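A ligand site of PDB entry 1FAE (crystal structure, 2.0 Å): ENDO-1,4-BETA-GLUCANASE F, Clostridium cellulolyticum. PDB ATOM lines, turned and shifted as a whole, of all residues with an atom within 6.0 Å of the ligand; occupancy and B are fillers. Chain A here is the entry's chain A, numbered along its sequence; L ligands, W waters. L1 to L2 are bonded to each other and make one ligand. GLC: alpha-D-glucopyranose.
An oxygen (O3) of GLC L2 is in hydrogen-bond range of the side-chain carboxylate (OE1) of Glu 55, at 2.6 Å.
The side-chain carboxylate (OE2) of Glu 44 is in hydrogen-bond range of an oxygen (O2) of GLC L2 (2.6 Å).
The side-chain carboxylate (OD2) of Asp 494 is in hydrogen-bond range of an oxygen (O6) of GLC L1.
O2 of GLC L2 sits at hydrogen-bond distance from NE1 of Trp 611.
Merely in contact with the ligand: His 36 (3.3 Å), Trp 411 (3.4 Å), Trp 417 (3.7 Å) and Arg 609 (3.4 Å).
Hydrophobic or aromatic side chains that line the ligand: His 36, Trp 411, Trp 417 and Trp 611.
Within 4 Å of the ligand: His 36, Glu 44, Glu 55, Trp 411, Trp 417, Asp 494, Arg 609 and Trp 611.
The nearest printed residue that does not touch the ligand is Ala 45 (4.1 Å).
Water W2 lies within hydrogen-bond range of an oxygen (O4) of GLC L2 (2.6 Å) and the side-chain carboxylate (OE2) of Glu 55 (3.1 Å).
Water W1 lies within hydrogen-bond range of an oxygen (O6) of GLC L2 (2.7 Å) and the backbone carbonyl oxygen of Glu 44 (2.7 Å).
Water W4 lies within hydrogen-bond range of the side-chain carboxylate (OD2) of Asp 494, the indole nitrogen (NE1) of Trp 411 and an oxygen (O1) of GLC L1.
Water W6 lies within hydrogen-bond range of the side-chain carboxylate of Asp 494 (2.7 Å) and an oxygen (O6) of GLC L1 (3.4 Å).
OG1 of Thr 53 sits close to N of Glu 55, at 3.5 Å.
A ring nitrogen (NE2) of His 36 sits at hydrogen-bond distance from the side-chain carboxylate (OE2) of Glu 44 (2.9 Å).
NE of Arg 609 lies within salt-bridge range of OE2 of Glu 44.
OE1 of Glu 44 is in salt-bridge range of NH2 of Arg 544, 3.2 Å away.
The backbone NH (N) of Cys 497 lies within hydrogen-bond range of the side-chain carboxylate (OD1) of Asp 494, 3.1 Å away.
The side-chain carboxylate (OE2) of Glu 542 is in salt-bridge range of the guanidinium group (NH1) of Arg 609 (2.9 Å).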
ATOM      1  N   HIS A  36      27.640 -23.138  26.483  1.00  0.00           N
ATOM      2  CA  HIS A  36      26.197 -22.872  26.533  1.00  0.00           C
ATOM      3  C   HIS A  36      25.821 -22.084  25.263  1.00  0.00           C
ATOM      4  O   HIS A  36      24.775 -22.321  24.670  1.00  0.00           O
ATOM      5  CB  HIS A  36      25.825 -22.070  27.784  1.00  0.00           C
ATOM      6  CG  HIS A  36      24.384 -21.673  27.836  1.00  0.00           C
ATOM      7  ND1 HIS A  36      23.380 -22.537  28.208  1.00  0.00           N
ATOM      8  CD2 HIS A  36      23.768 -20.500  27.546  1.00  0.00           C
ATOM      9  CE1 HIS A  36      22.216 -21.923  28.134  1.00  0.00           C
ATOM     10  NE2 HIS A  36      22.419 -20.677  27.739  1.00  0.00           N
ATOM     11  N   GLU A  44      21.111 -16.284  32.033  1.00  0.00           N
ATOM     12  CA  GLU A  44      19.734 -16.780  31.993  1.00  0.00           C
ATOM     13  C   GLU A  44      19.463 -17.954  32.932  1.00  0.00           C
ATOM     14  O   GLU A  44      18.393 -18.031  33.507  1.00  0.00           O
ATOM     15  CB  GLU A  44      19.278 -17.102  30.559  1.00  0.00           C
ATOM     16  CG  GLU A  44      20.142 -18.101  29.782  1.00  0.00           C
ATOM     17  CD  GLU A  44      19.809 -18.038  28.300  1.00  0.00           C
ATOM     18  OE1 GLU A  44      19.390 -16.968  27.829  1.00  0.00           O
ATOM     19  OE2 GLU A  44      19.951 -19.069  27.606  1.00  0.00           O
ATOM     20  N   ALA A  45      20.392 -18.899  32.989  1.00  0.00           N
ATOM     21  CA  ALA A  45      20.352 -20.068  33.912  1.00  0.00           C
ATOM     22  C   ALA A  45      21.855 -20.009  34.247  1.00  0.00           C
ATOM     23  O   ALA A  45      22.223 -19.787  35.396  1.00  0.00           O
ATOM     24  CB  ALA A  45      19.934 -21.352  33.201  1.00  0.00           C
ATOM     25  N   PRO A  46      22.747 -20.301  33.273  1.00  0.00           N
ATOM     26  CA  PRO A  46      24.143 -20.142  33.682  1.00  0.00           C
ATOM     27  C   PRO A  46      24.321 -18.596  33.602  1.00  0.00           C
ATOM     28  O   PRO A  46      23.472 -17.912  33.039  1.00  0.00           O
ATOM     29  CB  PRO A  46      24.915 -20.876  32.591  1.00  0.00           C
ATOM     30  CG  PRO A  46      24.030 -20.756  31.403  1.00  0.00           C
ATOM     31  CD  PRO A  46      22.679 -21.031  31.993  1.00  0.00           C
ATOM     32  N   THR A  53      26.783 -26.920  30.682  1.00  0.00           N
ATOM     33  CA  THR A  53      25.863 -27.563  31.611  1.00  0.00           C
ATOM     34  C   THR A  53      25.722 -29.020  31.195  1.00  0.00           C
ATOM     35  O   THR A  53      26.107 -29.390  30.080  1.00  0.00           O
ATOM     36  CB  THR A  53      24.462 -26.914  31.569  1.00  0.00           C
ATOM     37  OG1 THR A  53      23.976 -26.930  30.223  1.00  0.00           O
ATOM     38  CG2 THR A  53      24.505 -25.476  32.089  1.00  0.00           C
ATOM     39  N   GLU A  55      23.059 -30.251  30.614  1.00  0.00           N
ATOM     40  CA  GLU A  55      22.013 -30.106  29.605  1.00  0.00           C
ATOM     41  C   GLU A  55      22.668 -30.015  28.216  1.00  0.00           C
ATOM     42  O   GLU A  55      22.260 -30.727  27.293  1.00  0.00           O
ATOM     43  CB  GLU A  55      21.223 -28.828  29.905  1.00  0.00           C
ATOM     44  CG  GLU A  55      20.342 -28.348  28.780  1.00  0.00           C
ATOM     45  CD  GLU A  55      19.710 -27.012  29.134  1.00  0.00           C
ATOM     46  OE1 GLU A  55      20.179 -25.973  28.630  1.00  0.00           O
ATOM     47  OE2 GLU A  55      18.754 -27.024  29.937  1.00  0.00           O
ATOM     48  N   ASP A 230      16.917 -33.925  34.726  1.00  0.00           N
ATOM     49  CA  ASP A 230      16.358 -33.887  33.371  1.00  0.00           C
ATOM     50  C   ASP A 230      17.446 -34.117  32.303  1.00  0.00           C
ATOM     51  O   ASP A 230      17.176 -34.712  31.257  1.00  0.00           O
ATOM     52  CB  ASP A 230      15.591 -32.575  33.116  1.00  0.00           C
ATOM     53  CG  ASP A 230      16.470 -31.325  33.152  1.00  0.00           C
ATOM     54  OD1 ASP A 230      17.479 -31.275  33.891  1.00  0.00           O
ATOM     55  OD2 ASP A 230      16.142 -30.363  32.426  1.00  0.00           O
ATOM     56  N   PRO A 406      12.719 -15.793  37.714  1.00  0.00           N
ATOM     57  CA  PRO A 406      11.269 -15.811  37.488  1.00  0.00           C
ATOM     58  C   PRO A 406      10.663 -17.193  37.796  1.00  0.00           C
ATOM     59  O   PRO A 406      11.395 -18.154  38.062  1.00  0.00           O
ATOM     60  CB  PRO A 406      11.171 -15.491  35.998  1.00  0.00           C
ATOM     61  CG  PRO A 406      12.338 -16.243  35.438  1.00  0.00           C
ATOM     62  CD  PRO A 406      13.453 -15.983  36.442  1.00  0.00           C
ATOM     63  N   TRP A 411       8.001 -20.118  31.659  1.00  0.00           N
ATOM     64  CA  TRP A 411       8.704 -20.306  30.389  1.00  0.00           C
ATOM     65  C   TRP A 411       7.995 -21.413  29.603  1.00  0.00           C
ATOM     66  O   TRP A 411       7.829 -22.528  30.111  1.00  0.00           O
ATOM     67  CB  TRP A 411      10.150 -20.718  30.647  1.00  0.00           C
ATOM     68  CG  TRP A 411      10.993 -20.905  29.393  1.00  0.00           C
ATOM     69  CD1 TRP A 411      11.101 -20.024  28.352  1.00  0.00           C
ATOM     70  CD2 TRP A 411      11.829 -22.017  29.081  1.00  0.00           C
ATOM     71  NE1 TRP A 411      11.968 -20.530  27.406  1.00  0.00           N
ATOM     72  CE2 TRP A 411      12.429 -21.751  27.828  1.00  0.00           C
ATOM     73  CE3 TRP A 411      12.138 -23.223  29.735  1.00  0.00           C
ATOM     74  CZ2 TRP A 411      13.310 -22.646  27.203  1.00  0.00           C
ATOM     75  CZ3 TRP A 411      13.016 -24.115  29.119  1.00  0.00           C
ATOM     76  CH2 TRP A 411      13.593 -23.814  27.868  1.00  0.00           C
ATOM     77  N   MET A 414       9.381 -25.376  28.919  1.00  0.00           N
ATOM     78  CA  MET A 414       9.119 -26.555  29.739  1.00  0.00           C
ATOM     79  C   MET A 414       8.040 -27.416  29.095  1.00  0.00           C
ATOM     80  O   MET A 414       8.140 -28.646  29.109  1.00  0.00           O
ATOM     81  CB  MET A 414       8.744 -26.184  31.180  1.00  0.00           C
ATOM     82  CG  MET A 414       9.902 -25.606  31.986  1.00  0.00           C
ATOM     83  SD  MET A 414      11.248 -26.805  32.209  1.00  0.00           S
ATOM     84  CE  MET A 414      12.096 -26.102  33.559  1.00  0.00           C
ATOM     85  N   TRP A 417       9.842 -29.311  25.910  1.00  0.00           N
ATOM     86  CA  TRP A 417      10.891 -30.242  26.308  1.00  0.00           C
ATOM     87  C   TRP A 417      10.311 -31.518  26.936  1.00  0.00           C
ATOM     88  O   TRP A 417      10.682 -32.636  26.587  1.00  0.00           O
ATOM     89  CB  TRP A 417      11.827 -29.573  27.317  1.00  0.00           C
ATOM     90  CG  TRP A 417      12.898 -28.751  26.689  1.00  0.00           C
ATOM     91  CD1 TRP A 417      13.090 -28.536  25.345  1.00  0.00           C
ATOM     92  CD2 TRP A 417      13.969 -28.081  27.366  1.00  0.00           C
ATOM     93  NE1 TRP A 417      14.220 -27.778  25.152  1.00  0.00           N
ATOM     94  CE2 TRP A 417      14.784 -27.492  26.374  1.00  0.00           C
ATOM     95  CE3 TRP A 417      14.314 -27.932  28.708  1.00  0.00           C
ATOM     96  CZ2 TRP A 417      15.932 -26.757  26.687  1.00  0.00           C
ATOM     97  CZ3 TRP A 417      15.455 -27.220  29.017  1.00  0.00           C
ATOM     98  CH2 TRP A 417      16.252 -26.635  28.011  1.00  0.00           C
ATOM     99  N   SER A 461       5.545 -17.532  24.573  1.00  0.00           N
ATOM    100  CA  SER A 461       6.860 -17.306  25.166  1.00  0.00           C
ATOM    101  C   SER A 461       6.789 -17.357  26.688  1.00  0.00           C
ATOM    102  O   SER A 461       7.449 -18.172  27.333  1.00  0.00           O
ATOM    103  CB  SER A 461       7.395 -15.945  24.692  1.00  0.00           C
ATOM    104  OG  SER A 461       8.674 -15.731  25.225  1.00  0.00           O
ATOM    105  N   ASP A 494      11.319 -17.864  19.857  1.00  0.00           N
ATOM    106  CA  ASP A 494      12.432 -18.601  20.449  1.00  0.00           C
ATOM    107  C   ASP A 494      12.649 -19.820  19.540  1.00  0.00           C
ATOM    108  O   ASP A 494      11.810 -20.728  19.474  1.00  0.00           O
ATOM    109  CB  ASP A 494      12.077 -19.036  21.873  1.00  0.00           C
ATOM    110  CG  ASP A 494      13.245 -19.651  22.586  1.00  0.00           C
ATOM    111  OD1 ASP A 494      13.881 -20.579  22.041  1.00  0.00           O
ATOM    112  OD2 ASP A 494      13.545 -19.199  23.710  1.00  0.00           O
ATOM    113  N   CYS A 497      12.804 -23.366  21.305  1.00  0.00           N
ATOM    114  CA  CYS A 497      11.472 -23.820  21.695  1.00  0.00           C
ATOM    115  C   CYS A 497      10.643 -24.239  20.489  1.00  0.00           C
ATOM    116  O   CYS A 497       9.918 -25.215  20.561  1.00  0.00           O
ATOM    117  CB  CYS A 497      10.723 -22.733  22.489  1.00  0.00           C
ATOM    118  SG  CYS A 497      11.451 -22.380  24.109  1.00  0.00           S
ATOM    119  N   GLU A 542      16.700 -10.927  19.810  1.00  0.00           N
ATOM    120  CA  GLU A 542      15.799 -10.993  20.941  1.00  0.00           C
ATOM    121  C   GLU A 542      16.151  -9.927  21.959  1.00  0.00           C
ATOM    122  O   GLU A 542      17.297  -9.512  22.069  1.00  0.00           O
ATOM    123  CB  GLU A 542      15.851 -12.375  21.587  1.00  0.00           C
ATOM    124  CG  GLU A 542      17.166 -12.698  22.263  1.00  0.00           C
ATOM    125  CD  GLU A 542      17.182 -14.102  22.852  1.00  0.00           C
ATOM    126  OE1 GLU A 542      16.830 -14.274  24.044  1.00  0.00           O
ATOM    127  OE2 GLU A 542      17.520 -15.047  22.098  1.00  0.00           O
ATOM    128  N   ARG A 544      16.685  -8.583  25.717  1.00  0.00           N
ATOM    129  CA  ARG A 544      17.162  -9.139  26.985  1.00  0.00           C
ATOM    130  C   ARG A 544      16.625  -8.217  28.085  1.00  0.00           C
ATOM    131  O   ARG A 544      17.348  -7.372  28.626  1.00  0.00           O
ATOM    132  CB  ARG A 544      18.692  -9.200  26.997  1.00  0.00           C
ATOM    133  CG  ARG A 544      19.291  -9.828  25.748  1.00  0.00           C
ATOM    134  CD  ARG A 544      18.922 -11.292  25.584  1.00  0.00           C
ATOM    135  NE  ARG A 544      19.816 -12.160  26.338  1.00  0.00           N
ATOM    136  CZ  ARG A 544      19.451 -13.243  27.011  1.00  0.00           C
ATOM    137  NH1 ARG A 544      18.175 -13.628  27.043  1.00  0.00           N
ATOM    138  NH2 ARG A 544      20.364 -13.963  27.653  1.00  0.00           N
ATOM    139  N   ARG A 609      22.716 -20.404  21.045  1.00  0.00           N
ATOM    140  CA  ARG A 609      22.723 -21.341  22.175  1.00  0.00           C
ATOM    141  C   ARG A 609      22.913 -22.738  21.624  1.00  0.00           C
ATOM    142  O   ARG A 609      22.168 -23.158  20.743  1.00  0.00           O
ATOM    143  CB  ARG A 609      21.393 -21.270  22.929  1.00  0.00           C
ATOM    144  CG  ARG A 609      21.096 -19.926  23.551  1.00  0.00           C
ATOM    145  CD  ARG A 609      19.721 -19.940  24.171  1.00  0.00           C
ATOM    146  NE  ARG A 609      19.416 -18.697  24.889  1.00  0.00           N
ATOM    147  CZ  ARG A 609      18.883 -17.604  24.332  1.00  0.00           C
ATOM    148  NH1 ARG A 609      18.580 -17.586  23.033  1.00  0.00           N
ATOM    149  NH2 ARG A 609      18.590 -16.561  25.091  1.00  0.00           N
ATOM    150  N   TRP A 611      22.240 -25.755  22.738  1.00  0.00           N
ATOM    151  CA  TRP A 611      21.085 -26.606  22.806  1.00  0.00           C
ATOM    152  C   TRP A 611      20.052 -26.268  21.743  1.00  0.00           C
ATOM    153  O   TRP A 611      19.481 -27.184  21.150  1.00  0.00           O
ATOM    154  CB  TRP A 611      20.462 -26.605  24.210  1.00  0.00           C
ATOM    155  CG  TRP A 611      19.636 -25.412  24.591  1.00  0.00           C
ATOM    156  CD1 TRP A 611      20.017 -24.400  25.427  1.00  0.00           C
ATOM    157  CD2 TRP A 611      18.251 -25.181  24.292  1.00  0.00           C
ATOM    158  NE1 TRP A 611      18.956 -23.574  25.673  1.00  0.00           N
ATOM    159  CE2 TRP A 611      17.861 -24.025  25.000  1.00  0.00           C
ATOM    160  CE3 TRP A 611      17.292 -25.848  23.499  1.00  0.00           C
ATOM    161  CZ2 TRP A 611      16.545 -23.508  24.935  1.00  0.00           C
ATOM    162  CZ3 TRP A 611      15.998 -25.343  23.435  1.00  0.00           C
ATOM    163  CH2 TRP A 611      15.636 -24.186  24.150  1.00  0.00           C
HETATM  164  C1  GLC L   1      14.473 -16.709  27.648  1.00  0.00           C
HETATM  165  C2  GLC L   1      14.037 -17.415  28.928  1.00  0.00           C
HETATM  166  C3  GLC L   1      15.170 -18.307  29.433  1.00  0.00           C
HETATM  167  C4  GLC L   1      15.622 -19.255  28.309  1.00  0.00           C
HETATM  168  C5  GLC L   1      15.932 -18.483  27.023  1.00  0.00           C
HETATM  169  C6  GLC L   1      16.242 -19.384  25.840  1.00  0.00           C
HETATM  170  O1  GLC L   1      13.404 -15.972  27.169  1.00  0.00           O
HETATM  171  O2  GLC L   1      13.701 -16.462  29.914  1.00  0.00           O
HETATM  172  O3  GLC L   1      14.725 -19.065  30.553  1.00  0.00           O
HETATM  173  O4  GLC L   1      16.834 -19.893  28.731  1.00  0.00           O
HETATM  174  O5  GLC L   1      14.801 -17.666  26.650  1.00  0.00           O
HETATM  175  O6  GLC L   1      15.181 -20.283  25.586  1.00  0.00           O
HETATM  176  C1  GLC L   2      16.819 -21.259  28.903  1.00  0.00           C
HETATM  177  C2  GLC L   2      18.275 -21.716  28.971  1.00  0.00           C
HETATM  178  C3  GLC L   2      18.344 -23.210  29.287  1.00  0.00           C
HETATM  179  C4  GLC L   2      17.591 -23.443  30.607  1.00  0.00           C
HETATM  180  C5  GLC L   2      16.148 -22.926  30.474  1.00  0.00           C
HETATM  181  C6  GLC L   2      15.288 -23.099  31.717  1.00  0.00           C
HETATM  182  O2  GLC L   2      18.903 -21.447  27.725  1.00  0.00           O
HETATM  183  O3  GLC L   2      19.714 -23.570  29.425  1.00  0.00           O
HETATM  184  O4  GLC L   2      17.572 -24.826  30.920  1.00  0.00           O
HETATM  185  O5  GLC L   2      16.160 -21.538  30.146  1.00  0.00           O
HETATM  186  O6  GLC L   2      15.927 -22.556  32.863  1.00  0.00           O
HETATM  187  O   HOH W   1      16.450 -19.937  33.338  1.00  0.00           O
HETATM  188  O   HOH W   2      17.584 -26.643  32.730  1.00  0.00           O
HETATM  189  O   HOH W   3      18.428 -24.194  33.565  1.00  0.00           O
HETATM  190  O   HOH W   4      11.743 -18.242  25.352  1.00  0.00           O
HETATM  191  O   HOH W   5      12.529 -17.898  32.110  1.00  0.00           O
HETATM  192  O   HOH W   6      16.383 -21.301  22.608  1.00  0.00           O
HETATM  193  O   HOH W   7      15.275 -24.051  35.183  1.00  0.00           O
HETATM  194  O   HOH W   8      14.487 -16.447  23.597  1.00  0.00           O
